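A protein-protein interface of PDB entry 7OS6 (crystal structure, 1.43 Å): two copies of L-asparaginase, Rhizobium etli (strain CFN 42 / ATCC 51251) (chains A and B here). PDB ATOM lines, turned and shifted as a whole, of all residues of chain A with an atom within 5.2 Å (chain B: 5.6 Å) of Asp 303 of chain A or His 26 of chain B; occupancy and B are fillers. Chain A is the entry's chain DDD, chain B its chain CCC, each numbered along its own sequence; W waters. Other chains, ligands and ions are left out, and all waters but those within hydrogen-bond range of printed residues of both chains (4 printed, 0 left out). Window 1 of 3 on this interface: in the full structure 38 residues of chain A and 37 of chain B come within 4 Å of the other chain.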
ATOM      1  N   SER A  25      29.709 -22.779  -8.280  1.00  0.00           N
ATOM      2  CA  SER A  25      29.798 -21.735  -7.236  1.00  0.00           C
ATOM      3  C   SER A  25      28.909 -20.568  -7.654  1.00  0.00           C
ATOM      4  O   SER A  25      28.731 -20.314  -8.840  1.00  0.00           O
ATOM      5  CB  SER A  25      31.204 -21.315  -6.916  1.00  0.00           C
ATOM      6  OG  SER A  25      31.832 -20.675  -7.986  1.00  0.00           O
ATOM      7  N   HIS A  26      28.366 -19.919  -6.661  1.00  0.00           N
ATOM      8  CA  HIS A  26      27.382 -18.831  -6.836  1.00  0.00           C
ATOM      9  C   HIS A  26      27.807 -17.650  -5.977  1.00  0.00           C
ATOM     10  O   HIS A  26      27.920 -17.798  -4.766  1.00  0.00           O
ATOM     11  CB  HIS A  26      25.993 -19.321  -6.469  1.00  0.00           C
ATOM     12  CG  HIS A  26      25.567 -20.606  -7.099  1.00  0.00           C
ATOM     13  ND1 HIS A  26      24.716 -20.652  -8.174  1.00  0.00           N
ATOM     14  CD2 HIS A  26      25.846 -21.909  -6.798  1.00  0.00           C
ATOM     15  CE1 HIS A  26      24.469 -21.916  -8.487  1.00  0.00           C
ATOM     16  NE2 HIS A  26      25.130 -22.726  -7.663  1.00  0.00           N
ATOM     17  N   ARG A  27      27.967 -16.494  -6.595  1.00  0.00           N
ATOM     18  CA  ARG A  27      28.365 -15.284  -5.841  1.00  0.00           C
ATOM     19  C   ARG A  27      27.166 -14.719  -5.096  1.00  0.00           C
ATOM     20  O   ARG A  27      26.038 -14.649  -5.666  1.00  0.00           O
ATOM     21  CB  ARG A  27      28.904 -14.220  -6.800  1.00  0.00           C
ATOM     22  CG  ARG A  27      29.343 -12.985  -6.056  1.00  0.00           C
ATOM     23  CD  ARG A  27      30.007 -12.001  -7.012  1.00  0.00           C
ATOM     24  NE  ARG A  27      31.270 -12.429  -7.573  1.00  0.00           N
ATOM     25  CZ  ARG A  27      32.468 -12.330  -6.965  1.00  0.00           C
ATOM     26  NH1 ARG A  27      33.565 -12.709  -7.600  1.00  0.00           N
ATOM     27  NH2 ARG A  27      32.544 -11.906  -5.717  1.00  0.00           N
ATOM     28  N   ILE A 301      21.556 -13.546  -5.275  1.00  0.00           N
ATOM     29  CA  ILE A 301      22.470 -14.539  -5.893  1.00  0.00           C
ATOM     30  C   ILE A 301      22.785 -14.041  -7.297  1.00  0.00           C
ATOM     31  O   ILE A 301      21.838 -13.923  -8.115  1.00  0.00           O
ATOM     32  CB  ILE A 301      21.868 -15.952  -5.893  1.00  0.00           C
ATOM     33  CG1 ILE A 301      21.406 -16.408  -4.506  1.00  0.00           C
ATOM     34  CG2 ILE A 301      22.852 -16.920  -6.489  1.00  0.00           C
ATOM     35  CD1 ILE A 301      22.499 -16.459  -3.495  1.00  0.00           C
ATOM     36  N   GLU A 302      24.070 -13.736  -7.540  1.00  0.00           N
ATOM     37  CA  GLU A 302      24.472 -13.043  -8.787  1.00  0.00           C
ATOM     38  C   GLU A 302      23.921 -13.742 -10.040  1.00  0.00           C
ATOM     39  O   GLU A 302      23.504 -13.069 -11.008  1.00  0.00           O
ATOM     40  CB  GLU A 302      25.985 -12.912  -8.834  1.00  0.00           C
ATOM     41  CG  GLU A 302      26.481 -12.179 -10.056  1.00  0.00           C
ATOM     42  CD  GLU A 302      25.998 -10.757 -10.112  1.00  0.00           C
ATOM     43  OE1 GLU A 302      25.971 -10.122  -9.042  1.00  0.00           O
ATOM     44  OE2 GLU A 302      25.686 -10.244 -11.250  1.00  0.00           O
ATOM     45  N   ASP A 303      23.963 -15.072 -10.082  1.00  0.00           N
ATOM     46  CA  ASP A 303      23.582 -15.871 -11.245  1.00  0.00           C
ATOM     47  C   ASP A 303      22.089 -16.221 -11.262  1.00  0.00           C
ATOM     48  O   ASP A 303      21.627 -16.875 -12.238  1.00  0.00           O
ATOM     49  CB  ASP A 303      24.420 -17.150 -11.268  1.00  0.00           C
ATOM     50  CG  ASP A 303      24.319 -17.912  -9.968  1.00  0.00           C
ATOM     51  OD1 ASP A 303      23.394 -18.708  -9.842  1.00  0.00           O
ATOM     52  OD2 ASP A 303      25.149 -17.642  -9.119  1.00  0.00           O
ATOM     53  N   GLY A 304      21.302 -15.859 -10.227  1.00  0.00           N
ATOM     54  CA  GLY A 304      19.855 -16.052 -10.285  1.00  0.00           C
ATOM     55  C   GLY A 304      19.321 -17.376  -9.770  1.00  0.00           C
ATOM     56  O   GLY A 304      18.100 -17.643  -9.970  1.00  0.00           O
ATOM     57  N   ASN A 305      20.137 -18.214  -9.131  1.00  0.00           N
ATOM     58  CA  ASN A 305      19.674 -19.570  -8.735  1.00  0.00           C
ATOM     59  C   ASN A 305      18.815 -19.537  -7.455  1.00  0.00           C
ATOM     60  O   ASN A 305      19.350 -19.153  -6.375  1.00  0.00           O
ATOM     61  CB  ASN A 305      20.881 -20.477  -8.571  1.00  0.00           C
ATOM     62  CG  ASN A 305      20.489 -21.912  -8.300  1.00  0.00           C
ATOM     63  OD1 ASN A 305      19.958 -22.229  -7.259  1.00  0.00           O
ATOM     64  ND2 ASN A 305      20.765 -22.779  -9.273  1.00  0.00           N
ATOM     65  N   ASP B  12      35.402 -12.850 -17.568  1.00  0.00           N
ATOM     66  CA  ASP B  12      34.614 -13.331 -18.714  1.00  0.00           C
ATOM     67  C   ASP B  12      33.224 -13.772 -18.250  1.00  0.00           C
ATOM     68  O   ASP B  12      33.122 -14.738 -17.462  1.00  0.00           O
ATOM     69  CB  ASP B  12      35.377 -14.440 -19.421  1.00  0.00           C
ATOM     70  CG  ASP B  12      36.623 -13.931 -20.125  1.00  0.00           C
ATOM     71  OD1 ASP B  12      36.502 -12.922 -20.851  1.00  0.00           O
ATOM     72  OD2 ASP B  12      37.678 -14.566 -20.014  1.00  0.00           O
ATOM     73  N   PHE B  13      32.192 -13.080 -18.719  1.00  0.00           N
ATOM     74  CA  PHE B  13      30.798 -13.329 -18.285  1.00  0.00           C
ATOM     75  C   PHE B  13      29.850 -13.451 -19.455  1.00  0.00           C
ATOM     76  O   PHE B  13      30.061 -12.895 -20.542  1.00  0.00           O
ATOM     77  CB  PHE B  13      30.326 -12.187 -17.375  1.00  0.00           C
ATOM     78  CG  PHE B  13      30.985 -12.197 -16.020  1.00  0.00           C
ATOM     79  CD1 PHE B  13      32.250 -11.670 -15.831  1.00  0.00           C
ATOM     80  CD2 PHE B  13      30.390 -12.863 -14.965  1.00  0.00           C
ATOM     81  CE1 PHE B  13      32.882 -11.800 -14.604  1.00  0.00           C
ATOM     82  CE2 PHE B  13      31.006 -12.950 -13.726  1.00  0.00           C
ATOM     83  CZ  PHE B  13      32.249 -12.414 -13.547  1.00  0.00           C
ATOM     84  N   VAL B  14      28.730 -14.109 -19.200  1.00  0.00           N
ATOM     85  CA  VAL B  14      27.473 -13.998 -19.965  1.00  0.00           C
ATOM     86  C   VAL B  14      26.468 -13.338 -19.044  1.00  0.00           C
ATOM     87  O   VAL B  14      26.425 -13.651 -17.842  1.00  0.00           O
ATOM     88  CB  VAL B  14      27.028 -15.335 -20.586  1.00  0.00           C
ATOM     89  CG1 VAL B  14      26.869 -16.427 -19.542  1.00  0.00           C
ATOM     90  CG2 VAL B  14      25.755 -15.171 -21.388  1.00  0.00           C
ATOM     91  N   VAL B  15      25.692 -12.403 -19.570  1.00  0.00           N
ATOM     92  CA  VAL B  15      24.847 -11.502 -18.735  1.00  0.00           C
ATOM     93  C   VAL B  15      23.441 -11.487 -19.313  1.00  0.00           C
ATOM     94  O   VAL B  15      23.292 -11.406 -20.551  1.00  0.00           O
ATOM     95  CB  VAL B  15      25.501 -10.113 -18.662  1.00  0.00           C
ATOM     96  CG1 VAL B  15      24.651  -9.050 -18.020  1.00  0.00           C
ATOM     97  CG2 VAL B  15      26.839 -10.175 -17.962  1.00  0.00           C
ATOM     98  N   THR B  16      22.442 -11.428 -18.465  1.00  0.00           N
ATOM     99  CA  THR B  16      21.068 -11.130 -18.900  1.00  0.00           C
ATOM    100  C   THR B  16      20.732  -9.742 -18.375  1.00  0.00           C
ATOM    101  O   THR B  16      21.201  -9.334 -17.285  1.00  0.00           O
ATOM    102  CB  THR B  16      20.037 -12.178 -18.492  1.00  0.00           C
ATOM    103  OG1 THR B  16      20.086 -12.298 -17.068  1.00  0.00           O
ATOM    104  CG2 THR B  16      20.273 -13.494 -19.209  1.00  0.00           C
ATOM    105  N   ASN B  24      21.144 -11.014 -14.182  1.00  0.00           N
ATOM    106  CA  ASN B  24      22.068 -12.058 -13.700  1.00  0.00           C
ATOM    107  C   ASN B  24      23.361 -11.956 -14.478  1.00  0.00           C
ATOM    108  O   ASN B  24      23.335 -11.600 -15.685  1.00  0.00           O
ATOM    109  CB  ASN B  24      21.493 -13.456 -13.853  1.00  0.00           C
ATOM    110  CG  ASN B  24      20.166 -13.619 -13.176  1.00  0.00           C
ATOM    111  OD1 ASN B  24      19.938 -13.079 -12.102  1.00  0.00           O
ATOM    112  ND2 ASN B  24      19.315 -14.414 -13.775  1.00  0.00           N
ATOM    113  N   SER B  25      24.447 -12.344 -13.856  1.00  0.00           N
ATOM    114  CA  SER B  25      25.716 -12.574 -14.577  1.00  0.00           C
ATOM    115  C   SER B  25      26.248 -13.945 -14.223  1.00  0.00           C
ATOM    116  O   SER B  25      26.034 -14.439 -13.102  1.00  0.00           O
ATOM    117  CB  SER B  25      26.729 -11.497 -14.332  1.00  0.00           C
ATOM    118  OG  SER B  25      27.243 -11.468 -13.018  1.00  0.00           O
ATOM    119  N   HIS B  26      26.953 -14.529 -15.169  1.00  0.00           N
ATOM    120  CA  HIS B  26      27.423 -15.920 -15.069  1.00  0.00           C
ATOM    121  C   HIS B  26      28.869 -15.964 -15.546  1.00  0.00           C
ATOM    122  O   HIS B  26      29.133 -15.582 -16.689  1.00  0.00           O
ATOM    123  CB  HIS B  26      26.560 -16.837 -15.910  1.00  0.00           C
ATOM    124  CG  HIS B  26      25.087 -16.711 -15.720  1.00  0.00           C
ATOM    125  ND1 HIS B  26      24.383 -17.638 -14.993  1.00  0.00           N
ATOM    126  CD2 HIS B  26      24.163 -15.813 -16.191  1.00  0.00           C
ATOM    127  CE1 HIS B  26      23.090 -17.300 -15.002  1.00  0.00           C
ATOM    128  NE2 HIS B  26      22.912 -16.219 -15.748  1.00  0.00           N
ATOM    129  N   ARG B  27      29.766 -16.460 -14.728  1.00  0.00           N
ATOM    130  CA  ARG B  27      31.178 -16.574 -15.113  1.00  0.00           C
ATOM    131  C   ARG B  27      31.361 -17.749 -16.083  1.00  0.00           C
ATOM    132  O   ARG B  27      30.819 -18.861 -15.876  1.00  0.00           O
ATOM    133  CB  ARG B  27      32.058 -16.779 -13.886  1.00  0.00           C
ATOM    134  CG  ARG B  27      33.525 -16.875 -14.230  1.00  0.00           C
ATOM    135  CD  ARG B  27      34.395 -16.885 -13.007  1.00  0.00           C
ATOM    136  NE  ARG B  27      34.358 -15.690 -12.179  1.00  0.00           N
ATOM    137  CZ  ARG B  27      35.056 -14.561 -12.349  1.00  0.00           C
ATOM    138  NH1 ARG B  27      35.862 -14.429 -13.390  1.00  0.00           N
ATOM    139  NH2 ARG B  27      34.922 -13.568 -11.494  1.00  0.00           N
ATOM    140  N   VAL B  28      32.124 -17.508 -17.120  1.00  0.00           N
ATOM    141  CA  VAL B  28      32.395 -18.451 -18.225  1.00  0.00           C
ATOM    142  C   VAL B  28      33.846 -18.898 -18.176  1.00  0.00           C
ATOM    143  O   VAL B  28      34.760 -18.041 -18.053  1.00  0.00           O
ATOM    144  CB  VAL B  28      32.103 -17.823 -19.602  1.00  0.00           C
ATOM    145  CG1 VAL B  28      32.423 -18.803 -20.717  1.00  0.00           C
ATOM    146  CG2 VAL B  28      30.647 -17.398 -19.705  1.00  0.00           C
ATOM    147  N   ILE B 301      30.019 -23.177 -17.364  1.00  0.00           N
ATOM    148  CA  ILE B 301      29.355 -22.022 -16.716  1.00  0.00           C
ATOM    149  C   ILE B 301      29.495 -22.250 -15.210  1.00  0.00           C
ATOM    150  O   ILE B 301      28.986 -23.270 -14.693  1.00  0.00           O
ATOM    151  CB  ILE B 301      27.894 -21.896 -17.156  1.00  0.00           C
ATOM    152  CG1 ILE B 301      27.719 -21.836 -18.680  1.00  0.00           C
ATOM    153  CG2 ILE B 301      27.284 -20.671 -16.485  1.00  0.00           C
ATOM    154  CD1 ILE B 301      28.442 -20.709 -19.354  1.00  0.00           C
ATOM    155  N   ASP B 303      28.265 -21.263 -12.437  1.00  0.00           N
ATOM    156  CA  ASP B 303      27.076 -21.452 -11.572  1.00  0.00           C
ATOM    157  C   ASP B 303      26.155 -22.558 -12.092  1.00  0.00           C
ATOM    158  O   ASP B 303      25.153 -22.835 -11.426  1.00  0.00           O
ATOM    159  CB  ASP B 303      26.327 -20.120 -11.483  1.00  0.00           C
ATOM    160  CG  ASP B 303      26.010 -19.573 -12.880  1.00  0.00           C
ATOM    161  OD1 ASP B 303      24.978 -19.971 -13.456  1.00  0.00           O
ATOM    162  OD2 ASP B 303      26.825 -18.896 -13.442  1.00  0.00           O
ATOM    163  N   ASN B 305      24.247 -22.858 -15.025  1.00  0.00           N
ATOM    164  CA  ASN B 305      23.016 -22.548 -15.780  1.00  0.00           C
ATOM    165  C   ASN B 305      23.073 -23.081 -17.218  1.00  0.00           C
ATOM    166  O   ASN B 305      23.924 -22.610 -17.997  1.00  0.00           O
ATOM    167  CB  ASN B 305      22.780 -21.050 -15.742  1.00  0.00           C
ATOM    168  CG  ASN B 305      21.446 -20.671 -16.353  1.00  0.00           C
ATOM    169  OD1 ASN B 305      21.282 -20.748 -17.538  1.00  0.00           O
ATOM    170  ND2 ASN B 305      20.526 -20.195 -15.526  1.00  0.00           N
ATOM    171  N   MET B 308      22.239 -20.529 -20.256  1.00  0.00           N
ATOM    172  CA  MET B 308      23.444 -19.701 -20.516  1.00  0.00           C
ATOM    173  C   MET B 308      24.518 -20.525 -21.218  1.00  0.00           C
ATOM    174  O   MET B 308      25.169 -20.009 -22.151  1.00  0.00           O
ATOM    175  CB  MET B 308      23.972 -19.108 -19.221  1.00  0.00           C
ATOM    176  CG  MET B 308      23.014 -18.108 -18.609  1.00  0.00           C
ATOM    177  SD  MET B 308      22.617 -16.651 -19.618  1.00  0.00           S
ATOM    178  CE  MET B 308      21.051 -17.122 -20.283  1.00  0.00           C
HETATM  179  O   HOH W   1      22.746 -20.282 -11.987  1.00  0.00           O
HETATM  180  O   HOH W   2      32.713 -14.186  -9.947  1.00  0.00           O
HETATM  181  O   HOH W   3      22.715 -23.883 -11.449  1.00  0.00           O
HETATM  182  O   HOH W   4      20.444 -19.320 -12.845  1.00  0.00           O
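The side-chain carboxylate of Glu 302 of chain A sits at hydrogen-bond distance from the side-chain hydroxyl of Ser 25 of chain B, 2.7 Å away.
The backbone NH (N) of Asn 305 of chain B sits close to the side-chain carboxylate (OD1) of Asp 303 of chain B (3.4 Å).
O of Asn 24 of chain B is in hydrogen-bond range of N of Thr 16 of chain B.
N of His 26 of chain B lies within hydrogen-bond range of O of Val 14 of chain B, at 2.9 Å.
OD1 of Asp 303 of chain B is in hydrogen-bond range of ND1 of His 26 of chain B, 2.9 Å away.
OD1 of Asp 303 of chain A sits close to N of Asn 305 of chain A.
O of Arg 27 of chain A lies within hydrogen-bond range of N of Glu 302 of chain A, 2.9 Å away.
Among the printed residues, pairs that only touch across the chains: Ser 25 of chain A with Asp 303 of chain B (3.4 Å), His 26 of chain A with Asp 303 of chain B (3.2 Å), Glu 302 of chain A with Asn 24 of chain B (3.2 Å), Asp 303 of chain A with Asn 24 of chain B (3.7 Å), Asp 303 of chain A with Ser 25 of chain B (3.4 Å), Asp 303 of chain A with His 26 of chain B (3.2 Å), Asp 303 of chain A with Asp 303 of chain B (3.3 Å) and Gly 304 of chain A with Asn 24 of chain B (3.5 Å).
Arg 27 of chain A touches none of the printed residues of chain B.
Of chain B, only Asn 24, Ser 25, His 26 and Asp 303 come within 4 Å of Asp 303 of chain A.
Of the printed residues of chain B, Gly 304 of chain A touches Asn 24.
Of the printed residues of chain A, Asn 24 of chain B touches Glu 302 (3.2 Å), Asp 303 (3.7 Å) and Gly 304 (3.5 Å).
Printed residues of chain A within 4 Å of Ser 25 of chain B: Glu 302 (2.7 Å) and Asp 303 (3.4 Å).
The nearest printed residue of chain A that does not touch His 26 of chain B is Gly 304 of chain A (5.3 Å).
Of the 14 printed residues of chain B, 4 touch a printed residue of chain A.
Printed residues of chain B that touch a printed residue of chain A: Asn 24, Ser 25, His 26 and Asp 303.
Hydrophobic or aromatic side chains of chain B within 4 Å of the printed part of chain A: His 26.
Printed residues of chain A that touch a printed residue of chain B: Ser 25, His 26, Glu 302, Asp 303 and Gly 304.
Hydrophobic or aromatic side chains of chain A within 4 Å of the printed part of chain B: His 26.
Along chain A the printed residues that touch a printed residue of chain B span positions 25 to 304.
Among the printed residues, 9 pairs touch across the chains.
Among the printed residues, no Asp or Glu carboxylate lies within 4 Å of a Lys or Arg side-chain nitrogen of the other chain.
Ser 25 of chain A touches Asp 303 of chain B, and with the chains exchanged Asp 303 of chain A touches Ser 25 of chain B.
His 26 of chain A touches Asp 303 of chain B, and with the chains exchanged Asp 303 of chain A touches His 26 of chain B.
Asp 303 of chain A touches its own counterpart, Asp 303 of chain B.
Positions printed for both chains: 25, 26, 27, 301, 303 and 305.
Of the 9 pairs that touch across the chains among the printed residues, 5 have their exchanged pair printed and touching as well.
Water W3 lies within hydrogen-bond range of O of Asp 303 of chain B (2.7 Å) and ND2 of Asn 305 of chain A (3.1 Å).
Water W1 lies within hydrogen-bond range of the side-chain carboxylate of Asp 303 of chain B and the side-chain carboxylate of Asp 303 of chain A.
Water W2 lies within hydrogen-bond range of NH2 of Arg 27 of chain B (2.8 Å) and NH1 of Arg 27 of chain A (2.9 Å).
Water W4 bridges the backbone carbonyl oxygen (O) of Asp 303 of chain A (2.8 Å) and the side-chain amide nitrogen (ND2) of Asn 305 of chain B (2.8 Å).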
